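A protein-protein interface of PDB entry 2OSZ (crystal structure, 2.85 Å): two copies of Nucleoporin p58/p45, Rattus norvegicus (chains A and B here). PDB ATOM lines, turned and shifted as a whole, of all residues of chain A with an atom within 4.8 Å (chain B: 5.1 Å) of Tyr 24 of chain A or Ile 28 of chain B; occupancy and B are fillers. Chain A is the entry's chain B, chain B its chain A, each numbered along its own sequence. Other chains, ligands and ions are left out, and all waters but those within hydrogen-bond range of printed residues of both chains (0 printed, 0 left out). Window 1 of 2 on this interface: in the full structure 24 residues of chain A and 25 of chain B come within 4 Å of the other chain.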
ATOM      1  N   GLN A  20      -8.148   4.462   0.072  1.00  0.00           N
ATOM      2  CA  GLN A  20      -8.282   3.130   0.652  1.00  0.00           C
ATOM      3  C   GLN A  20      -7.463   2.078  -0.089  1.00  0.00           C
ATOM      4  O   GLN A  20      -6.801   1.248   0.531  1.00  0.00           O
ATOM      5  CB  GLN A  20      -9.752   2.712   0.677  1.00  0.00           C
ATOM      6  CG  GLN A  20     -10.521   3.328   1.811  1.00  0.00           C
ATOM      7  CD  GLN A  20      -9.632   3.569   3.008  1.00  0.00           C
ATOM      8  OE1 GLN A  20      -8.941   4.587   3.075  1.00  0.00           O
ATOM      9  NE2 GLN A  20      -9.616   2.623   3.948  1.00  0.00           N
ATOM     10  N   LEU A  21      -7.526   2.122  -1.417  1.00  0.00           N
ATOM     11  CA  LEU A  21      -6.798   1.192  -2.267  1.00  0.00           C
ATOM     12  C   LEU A  21      -5.288   1.367  -2.074  1.00  0.00           C
ATOM     13  O   LEU A  21      -4.549   0.391  -1.971  1.00  0.00           O
ATOM     14  CB  LEU A  21      -7.181   1.418  -3.728  1.00  0.00           C
ATOM     15  CG  LEU A  21      -6.954   0.207  -4.622  1.00  0.00           C
ATOM     16  CD1 LEU A  21      -7.682  -0.978  -4.018  1.00  0.00           C
ATOM     17  CD2 LEU A  21      -7.466   0.466  -6.022  1.00  0.00           C
ATOM     18  N   GLN A  22      -4.834   2.614  -2.016  1.00  0.00           N
ATOM     19  CA  GLN A  22      -3.417   2.886  -1.813  1.00  0.00           C
ATOM     20  C   GLN A  22      -3.025   2.252  -0.472  1.00  0.00           C
ATOM     21  O   GLN A  22      -2.107   1.435  -0.411  1.00  0.00           O
ATOM     22  CB  GLN A  22      -3.164   4.398  -1.793  1.00  0.00           C
ATOM     23  CG  GLN A  22      -1.707   4.846  -2.046  1.00  0.00           C
ATOM     24  CD  GLN A  22      -1.345   5.049  -3.540  1.00  0.00           C
ATOM     25  OE1 GLN A  22      -0.494   5.891  -3.876  1.00  0.00           O
ATOM     26  NE2 GLN A  22      -1.971   4.268  -4.428  1.00  0.00           N
ATOM     27  N   GLN A  23      -3.736   2.611   0.595  1.00  0.00           N
ATOM     28  CA  GLN A  23      -3.463   2.055   1.918  1.00  0.00           C
ATOM     29  C   GLN A  23      -3.450   0.516   1.920  1.00  0.00           C
ATOM     30  O   GLN A  23      -2.710  -0.111   2.684  1.00  0.00           O
ATOM     31  CB  GLN A  23      -4.500   2.562   2.921  1.00  0.00           C
ATOM     32  CG  GLN A  23      -4.150   3.896   3.564  1.00  0.00           C
ATOM     33  CD  GLN A  23      -5.271   4.452   4.452  1.00  0.00           C
ATOM     34  OE1 GLN A  23      -5.779   3.767   5.351  1.00  0.00           O
ATOM     35  NE2 GLN A  23      -5.654   5.706   4.204  1.00  0.00           N
ATOM     36  N   TYR A  24      -4.275  -0.089   1.067  1.00  0.00           N
ATOM     37  CA  TYR A  24      -4.358  -1.540   0.973  1.00  0.00           C
ATOM     38  C   TYR A  24      -3.077  -2.080   0.345  1.00  0.00           C
ATOM     39  O   TYR A  24      -2.445  -2.987   0.890  1.00  0.00           O
ATOM     40  CB  TYR A  24      -5.581  -1.946   0.137  1.00  0.00           C
ATOM     41  CG  TYR A  24      -5.757  -3.439  -0.075  1.00  0.00           C
ATOM     42  CD1 TYR A  24      -5.775  -4.327   1.008  1.00  0.00           C
ATOM     43  CD2 TYR A  24      -5.886  -3.967  -1.355  1.00  0.00           C
ATOM     44  CE1 TYR A  24      -5.909  -5.707   0.812  1.00  0.00           C
ATOM     45  CE2 TYR A  24      -6.022  -5.335  -1.561  1.00  0.00           C
ATOM     46  CZ  TYR A  24      -6.027  -6.203  -0.477  1.00  0.00           C
ATOM     47  OH  TYR A  24      -6.103  -7.566  -0.690  1.00  0.00           O
ATOM     48  N   ARG A  25      -2.696  -1.513  -0.800  1.00  0.00           N
ATOM     49  CA  ARG A  25      -1.486  -1.937  -1.502  1.00  0.00           C
ATOM     50  C   ARG A  25      -0.256  -1.848  -0.590  1.00  0.00           C
ATOM     51  O   ARG A  25       0.651  -2.666  -0.683  1.00  0.00           O
ATOM     52  CB  ARG A  25      -1.269  -1.076  -2.750  1.00  0.00           C
ATOM     53  CG  ARG A  25      -0.081  -1.513  -3.601  1.00  0.00           C
ATOM     54  CD  ARG A  25       0.507  -0.338  -4.395  1.00  0.00           C
ATOM     55  NE  ARG A  25       1.134   0.664  -3.526  1.00  0.00           N
ATOM     56  CZ  ARG A  25       0.785   1.947  -3.492  1.00  0.00           C
ATOM     57  NH1 ARG A  25      -0.183   2.384  -4.282  1.00  0.00           N
ATOM     58  NH2 ARG A  25       1.381   2.789  -2.655  1.00  0.00           N
ATOM     59  N   GLN A  26      -0.229  -0.859   0.296  1.00  0.00           N
ATOM     60  CA  GLN A  26       0.904  -0.705   1.193  1.00  0.00           C
ATOM     61  C   GLN A  26       0.995  -1.838   2.184  1.00  0.00           C
ATOM     62  O   GLN A  26       2.066  -2.403   2.376  1.00  0.00           O
ATOM     63  CB  GLN A  26       0.837   0.622   1.945  1.00  0.00           C
ATOM     64  CG  GLN A  26       0.957   1.820   1.030  1.00  0.00           C
ATOM     65  CD  GLN A  26       1.270   3.097   1.763  1.00  0.00           C
ATOM     66  OE1 GLN A  26       1.258   4.173   1.160  1.00  0.00           O
ATOM     67  NE2 GLN A  26       1.564   2.995   3.061  1.00  0.00           N
ATOM     68  N   GLN A  27      -0.116  -2.175   2.828  1.00  0.00           N
ATOM     69  CA  GLN A  27      -0.095  -3.280   3.781  1.00  0.00           C
ATOM     70  C   GLN A  27       0.415  -4.532   3.080  1.00  0.00           C
ATOM     71  O   GLN A  27       1.206  -5.273   3.652  1.00  0.00           O
ATOM     72  CB  GLN A  27      -1.487  -3.519   4.363  1.00  0.00           C
ATOM     73  CG  GLN A  27      -1.984  -2.351   5.194  1.00  0.00           C
ATOM     74  CD  GLN A  27      -3.438  -2.489   5.582  1.00  0.00           C
ATOM     75  OE1 GLN A  27      -4.272  -2.842   4.753  1.00  0.00           O
ATOM     76  NE2 GLN A  27      -3.754  -2.203   6.839  1.00  0.00           N
ATOM     77  N   ILE A  28      -0.017  -4.747   1.838  1.00  0.00           N
ATOM     78  CA  ILE A  28       0.408  -5.910   1.062  1.00  0.00           C
ATOM     79  C   ILE A  28       1.883  -5.832   0.680  1.00  0.00           C
ATOM     80  O   ILE A  28       2.538  -6.859   0.530  1.00  0.00           O
ATOM     81  CB  ILE A  28      -0.450  -6.080  -0.213  1.00  0.00           C
ATOM     82  CG1 ILE A  28      -1.830  -6.585   0.178  1.00  0.00           C
ATOM     83  CG2 ILE A  28       0.200  -7.065  -1.185  1.00  0.00           C
ATOM     84  CD1 ILE A  28      -2.798  -6.617  -0.974  1.00  0.00           C
ATOM     85  N   THR A  59      -6.543  -8.270   6.265  1.00  0.00           N
ATOM     86  CA  THR A  59      -6.276  -7.088   5.473  1.00  0.00           C
ATOM     87  C   THR A  59      -7.308  -6.867   4.353  1.00  0.00           C
ATOM     88  O   THR A  59      -7.560  -5.730   3.979  1.00  0.00           O
ATOM     89  CB  THR A  59      -4.843  -7.178   4.898  1.00  0.00           C
ATOM     90  OG1 THR A  59      -4.379  -5.873   4.566  1.00  0.00           O
ATOM     91  CG2 THR A  59      -4.811  -8.034   3.660  1.00  0.00           C
ATOM     92  N   PHE A  60      -7.903  -7.940   3.821  1.00  0.00           N
ATOM     93  CA  PHE A  60      -8.920  -7.835   2.752  1.00  0.00           C
ATOM     94  C   PHE A  60     -10.297  -7.434   3.305  1.00  0.00           C
ATOM     95  O   PHE A  60     -10.972  -6.567   2.755  1.00  0.00           O
ATOM     96  CB  PHE A  60      -9.052  -9.164   1.992  1.00  0.00           C
ATOM     97  CG  PHE A  60     -10.136  -9.160   0.946  1.00  0.00           C
ATOM     98  CD1 PHE A  60     -10.032  -8.354  -0.181  1.00  0.00           C
ATOM     99  CD2 PHE A  60     -11.294  -9.905   1.128  1.00  0.00           C
ATOM    100  CE1 PHE A  60     -11.064  -8.280  -1.109  1.00  0.00           C
ATOM    101  CE2 PHE A  60     -12.330  -9.840   0.210  1.00  0.00           C
ATOM    102  CZ  PHE A  60     -12.214  -9.020  -0.915  1.00  0.00           C
ATOM    103  N   LEU A  63     -10.478  -3.911   3.692  1.00  0.00           N
ATOM    104  CA  LEU A  63     -10.684  -3.186   2.441  1.00  0.00           C
ATOM    105  C   LEU A  63     -12.175  -3.278   2.077  1.00  0.00           C
ATOM    106  O   LEU A  63     -12.779  -2.317   1.602  1.00  0.00           O
ATOM    107  CB  LEU A  63      -9.836  -3.790   1.318  1.00  0.00           C
ATOM    108  CG  LEU A  63     -10.056  -3.185  -0.079  1.00  0.00           C
ATOM    109  CD1 LEU A  63      -9.602  -1.720  -0.120  1.00  0.00           C
ATOM    110  CD2 LEU A  63      -9.280  -3.982  -1.094  1.00  0.00           C
ATOM    111  N   TYR B  24      -0.253 -10.234  -7.219  1.00  0.00           N
ATOM    112  CA  TYR B  24      -1.445  -9.622  -6.662  1.00  0.00           C
ATOM    113  C   TYR B  24      -1.194  -8.126  -6.561  1.00  0.00           C
ATOM    114  O   TYR B  24      -1.875  -7.338  -7.209  1.00  0.00           O
ATOM    115  CB  TYR B  24      -1.759 -10.207  -5.285  1.00  0.00           C
ATOM    116  CG  TYR B  24      -3.030  -9.678  -4.665  1.00  0.00           C
ATOM    117  CD1 TYR B  24      -4.263  -9.856  -5.287  1.00  0.00           C
ATOM    118  CD2 TYR B  24      -3.002  -8.997  -3.453  1.00  0.00           C
ATOM    119  CE1 TYR B  24      -5.442  -9.366  -4.712  1.00  0.00           C
ATOM    120  CE2 TYR B  24      -4.170  -8.510  -2.870  1.00  0.00           C
ATOM    121  CZ  TYR B  24      -5.385  -8.696  -3.502  1.00  0.00           C
ATOM    122  OH  TYR B  24      -6.533  -8.224  -2.907  1.00  0.00           O
ATOM    123  N   ARG B  25      -0.197  -7.737  -5.773  1.00  0.00           N
ATOM    124  CA  ARG B  25       0.120  -6.324  -5.600  1.00  0.00           C
ATOM    125  C   ARG B  25       0.282  -5.578  -6.914  1.00  0.00           C
ATOM    126  O   ARG B  25       0.064  -4.374  -6.971  1.00  0.00           O
ATOM    127  CB  ARG B  25       1.396  -6.139  -4.790  1.00  0.00           C
ATOM    128  CG  ARG B  25       1.662  -4.675  -4.437  1.00  0.00           C
ATOM    129  CD  ARG B  25       3.136  -4.435  -4.289  1.00  0.00           C
ATOM    130  NE  ARG B  25       3.798  -4.780  -5.539  1.00  0.00           N
ATOM    131  CZ  ARG B  25       5.061  -5.166  -5.625  1.00  0.00           C
ATOM    132  NH1 ARG B  25       5.790  -5.249  -4.520  1.00  0.00           N
ATOM    133  NH2 ARG B  25       5.584  -5.474  -6.808  1.00  0.00           N
ATOM    134  N   GLN B  26       0.679  -6.286  -7.967  1.00  0.00           N
ATOM    135  CA  GLN B  26       0.870  -5.659  -9.268  1.00  0.00           C
ATOM    136  C   GLN B  26      -0.466  -5.341  -9.929  1.00  0.00           C
ATOM    137  O   GLN B  26      -0.647  -4.260 -10.489  1.00  0.00           O
ATOM    138  CB  GLN B  26       1.724  -6.556 -10.175  1.00  0.00           C
ATOM    139  CG  GLN B  26       3.209  -6.552  -9.817  1.00  0.00           C
ATOM    140  CD  GLN B  26       4.048  -7.492 -10.684  1.00  0.00           C
ATOM    141  OE1 GLN B  26       3.923  -7.514 -11.912  1.00  0.00           O
ATOM    142  NE2 GLN B  26       4.919  -8.261 -10.044  1.00  0.00           N
ATOM    143  N   GLN B  27      -1.407  -6.272  -9.863  1.00  0.00           N
ATOM    144  CA  GLN B  27      -2.705  -6.021 -10.459  1.00  0.00           C
ATOM    145  C   GLN B  27      -3.384  -4.875  -9.731  1.00  0.00           C
ATOM    146  O   GLN B  27      -4.076  -4.063 -10.336  1.00  0.00           O
ATOM    147  CB  GLN B  27      -3.563  -7.281 -10.417  1.00  0.00           C
ATOM    148  CG  GLN B  27      -3.072  -8.310 -11.398  1.00  0.00           C
ATOM    149  CD  GLN B  27      -3.958  -9.528 -11.487  1.00  0.00           C
ATOM    150  OE1 GLN B  27      -4.171 -10.231 -10.495  1.00  0.00           O
ATOM    151  NE2 GLN B  27      -4.474  -9.797 -12.688  1.00  0.00           N
ATOM    152  N   ILE B  28      -3.174  -4.796  -8.427  1.00  0.00           N
ATOM    153  CA  ILE B  28      -3.767  -3.725  -7.665  1.00  0.00           C
ATOM    154  C   ILE B  28      -3.096  -2.414  -8.042  1.00  0.00           C
ATOM    155  O   ILE B  28      -3.738  -1.368  -8.070  1.00  0.00           O
ATOM    156  CB  ILE B  28      -3.641  -4.019  -6.156  1.00  0.00           C
ATOM    157  CG1 ILE B  28      -4.748  -5.006  -5.769  1.00  0.00           C
ATOM    158  CG2 ILE B  28      -3.683  -2.718  -5.335  1.00  0.00           C
ATOM    159  CD1 ILE B  28      -4.685  -5.487  -4.359  1.00  0.00           C
ATOM    160  N   GLU B  29      -1.804  -2.485  -8.351  1.00  0.00           N
ATOM    161  CA  GLU B  29      -1.021  -1.318  -8.747  1.00  0.00           C
ATOM    162  C   GLU B  29      -1.483  -0.872 -10.121  1.00  0.00           C
ATOM    163  O   GLU B  29      -1.538   0.318 -10.422  1.00  0.00           O
ATOM    164  CB  GLU B  29       0.465  -1.668  -8.794  1.00  0.00           C
ATOM    165  CG  GLU B  29       1.261  -1.145  -7.618  1.00  0.00           C
ATOM    166  CD  GLU B  29       2.543  -1.939  -7.375  1.00  0.00           C
ATOM    167  OE1 GLU B  29       3.294  -2.212  -8.343  1.00  0.00           O
ATOM    168  OE2 GLU B  29       2.804  -2.286  -6.204  1.00  0.00           O
ATOM    169  N   GLU B  30      -1.815  -1.845 -10.958  1.00  0.00           N
ATOM    170  CA  GLU B  30      -2.295  -1.563 -12.302  1.00  0.00           C
ATOM    171  C   GLU B  30      -3.669  -0.899 -12.214  1.00  0.00           C
ATOM    172  O   GLU B  30      -3.919   0.121 -12.849  1.00  0.00           O
ATOM    173  CB  GLU B  30      -2.369  -2.868 -13.092  1.00  0.00           C
ATOM    174  CG  GLU B  30      -3.037  -2.774 -14.436  1.00  0.00           C
ATOM    175  CD  GLU B  30      -2.750  -3.999 -15.285  1.00  0.00           C
ATOM    176  OE1 GLU B  30      -3.416  -4.183 -16.334  1.00  0.00           O
ATOM    177  OE2 GLU B  30      -1.844  -4.778 -14.901  1.00  0.00           O
ATOM    178  N   LEU B  31      -4.549  -1.471 -11.398  1.00  0.00           N
ATOM    179  CA  LEU B  31      -5.896  -0.947 -11.225  1.00  0.00           C
ATOM    180  C   LEU B  31      -5.876   0.455 -10.629  1.00  0.00           C
ATOM    181  O   LEU B  31      -6.797   1.233 -10.851  1.00  0.00           O
ATOM    182  CB  LEU B  31      -6.721  -1.908 -10.348  1.00  0.00           C
ATOM    183  CG  LEU B  31      -8.219  -1.692 -10.080  1.00  0.00           C
ATOM    184  CD1 LEU B  31      -8.409  -0.965  -8.762  1.00  0.00           C
ATOM    185  CD2 LEU B  31      -8.858  -0.938 -11.235  1.00  0.00           C
ATOM    186  N   GLU B  32      -4.831   0.779  -9.874  1.00  0.00           N
ATOM    187  CA  GLU B  32      -4.721   2.113  -9.284  1.00  0.00           C
ATOM    188  C   GLU B  32      -4.312   3.117 -10.344  1.00  0.00           C
ATOM    189  O   GLU B  32      -4.856   4.206 -10.426  1.00  0.00           O
ATOM    190  CB  GLU B  32      -3.681   2.148  -8.168  1.00  0.00           C
ATOM    191  CG  GLU B  32      -4.118   1.525  -6.878  1.00  0.00           C
ATOM    192  CD  GLU B  32      -3.185   1.884  -5.733  1.00  0.00           C
ATOM    193  OE1 GLU B  32      -1.976   1.564  -5.822  1.00  0.00           O
ATOM    194  OE2 GLU B  32      -3.662   2.487  -4.744  1.00  0.00           O
ATOM    195  N   ILE B  56     -11.570  -5.665  -8.370  1.00  0.00           N
ATOM    196  CA  ILE B  56     -10.906  -5.891  -7.088  1.00  0.00           C
ATOM    197  C   ILE B  56     -11.300  -7.254  -6.537  1.00  0.00           C
ATOM    198  O   ILE B  56     -10.432  -8.058  -6.216  1.00  0.00           O
ATOM    199  CB  ILE B  56     -11.297  -4.856  -6.017  1.00  0.00           C
ATOM    200  CG1 ILE B  56     -10.853  -3.453  -6.419  1.00  0.00           C
ATOM    201  CG2 ILE B  56     -10.662  -5.236  -4.695  1.00  0.00           C
ATOM    202  CD1 ILE B  56      -9.391  -3.176  -6.219  1.00  0.00           C
ATOM    203  N   THR B  59      -9.798  -9.989  -8.543  1.00  0.00           N
ATOM    204  CA  THR B  59      -8.381 -10.136  -8.265  1.00  0.00           C
ATOM    205  C   THR B  59      -8.126 -10.930  -6.978  1.00  0.00           C
ATOM    206  O   THR B  59      -7.244 -11.792  -6.927  1.00  0.00           O
ATOM    207  CB  THR B  59      -7.727  -8.742  -8.182  1.00  0.00           C
ATOM    208  OG1 THR B  59      -7.833  -8.095  -9.456  1.00  0.00           O
ATOM    209  CG2 THR B  59      -6.268  -8.852  -7.818  1.00  0.00           C
ATOM    210  N   PHE B  60      -8.897 -10.629  -5.939  1.00  0.00           N
ATOM    211  CA  PHE B  60      -8.769 -11.326  -4.664  1.00  0.00           C
ATOM    212  C   PHE B  60      -9.162 -12.800  -4.851  1.00  0.00           C
ATOM    213  O   PHE B  60      -8.506 -13.707  -4.335  1.00  0.00           O
ATOM    214  CB  PHE B  60      -9.669 -10.669  -3.615  1.00  0.00           C
ATOM    215  CG  PHE B  60      -9.698 -11.396  -2.305  1.00  0.00           C
ATOM    216  CD1 PHE B  60      -8.577 -11.426  -1.484  1.00  0.00           C
ATOM    217  CD2 PHE B  60     -10.837 -12.084  -1.907  1.00  0.00           C
ATOM    218  CE1 PHE B  60      -8.593 -12.128  -0.282  1.00  0.00           C
ATOM    219  CE2 PHE B  60     -10.864 -12.784  -0.712  1.00  0.00           C
ATOM    220  CZ  PHE B  60      -9.740 -12.809   0.099  1.00  0.00           C
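The side-chain carboxylate (OE2) of Glu 32 of chain B lies within hydrogen-bond range of the side-chain amide nitrogen (NE2) of Gln 22 of chain A, at 2.5 Å. The side-chain carboxylate of Glu 32 of chain B lies within salt-bridge range of the guanidinium group of Arg 25 of chain A (2.5 Å). OH of Tyr 24 of chain A lies close to OH of Tyr 24 of chain B (2.4 Å).
NE of Arg 25 of chain B lies within salt-bridge range of OE2 of Glu 29 of chain B (2.8 Å). The guanidinium group (NH1) of Arg 25 of chain A lies close to the side-chain amide nitrogen (NE2) of Gln 22 of chain A, at 2.6 Å.
Among the printed residues, pairs that only touch across the chains: Leu 21 of chain A with Leu 31 of chain B (3.2 Å), Leu 21 of chain A with Glu 32 of chain B (3.3 Å), Leu 21 of chain A with Ile 56 of chain B (3.5 Å), Tyr 24 of chain A with Ile 28 of chain B (3.1 Å), Arg 25 of chain A with Arg 25 of chain B (3.7 Å), Arg 25 of chain A with Ile 28 of chain B (3.9 Å), Arg 25 of chain A with Glu 29 of chain B (3.4 Å), Ile 28 of chain A with Tyr 24 of chain B (3.0 Å), Ile 28 of chain A with Arg 25 of chain B (3.9 Å) and Phe 60 of chain A with Phe 60 of chain B (3.4 Å).
Tyr 24 of chain A touches just these residues of chain B: Tyr 24 (2.4 Å) and Ile 28 (3.1 Å). Ile 28 of chain B touches just these residues of chain A: Tyr 24 and Arg 25. Printed residues of chain A within 4 Å of Glu 29 of chain B: Arg 25 (3.4 Å). Printed residues of chain A within 4 Å of Leu 31 of chain B: Leu 21. Of the printed residues of chain A, Glu 32 of chain B touches Leu 21, Gln 22 and Arg 25. Printed residues of chain A within 4 Å of Phe 60 of chain B: Phe 60 (3.4 Å). Printed residues of chain B within 4 Å of Phe 60 of chain A: Phe 60 (3.4 Å). Gln 26 of chain A touches none of the printed residues of chain B. Thr 59 of chain B touches none of the printed residues of chain A. The nearest printed residue of chain A that does not touch Glu 32 of chain B is Gln 23 of chain A (5.3 Å).
Of the 12 printed residues of chain A, 6 touch a printed residue of chain B. Hydrophobic or aromatic side chains of chain A that line the printed part of chain B: Leu 21, Tyr 24, Ile 28 and Phe 60.
Tyr 24 of chain B touches its own counterpart, Tyr 24 of chain A. Arg 25 of chain B touches its own counterpart, Arg 25 of chain A. Arg 25 of chain A touches Ile 28 of chain B, and with the chains exchanged Ile 28 of chain A touches Arg 25 of chain B. Phe 60 of chain B touches its own counterpart, Phe 60 of chain A.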
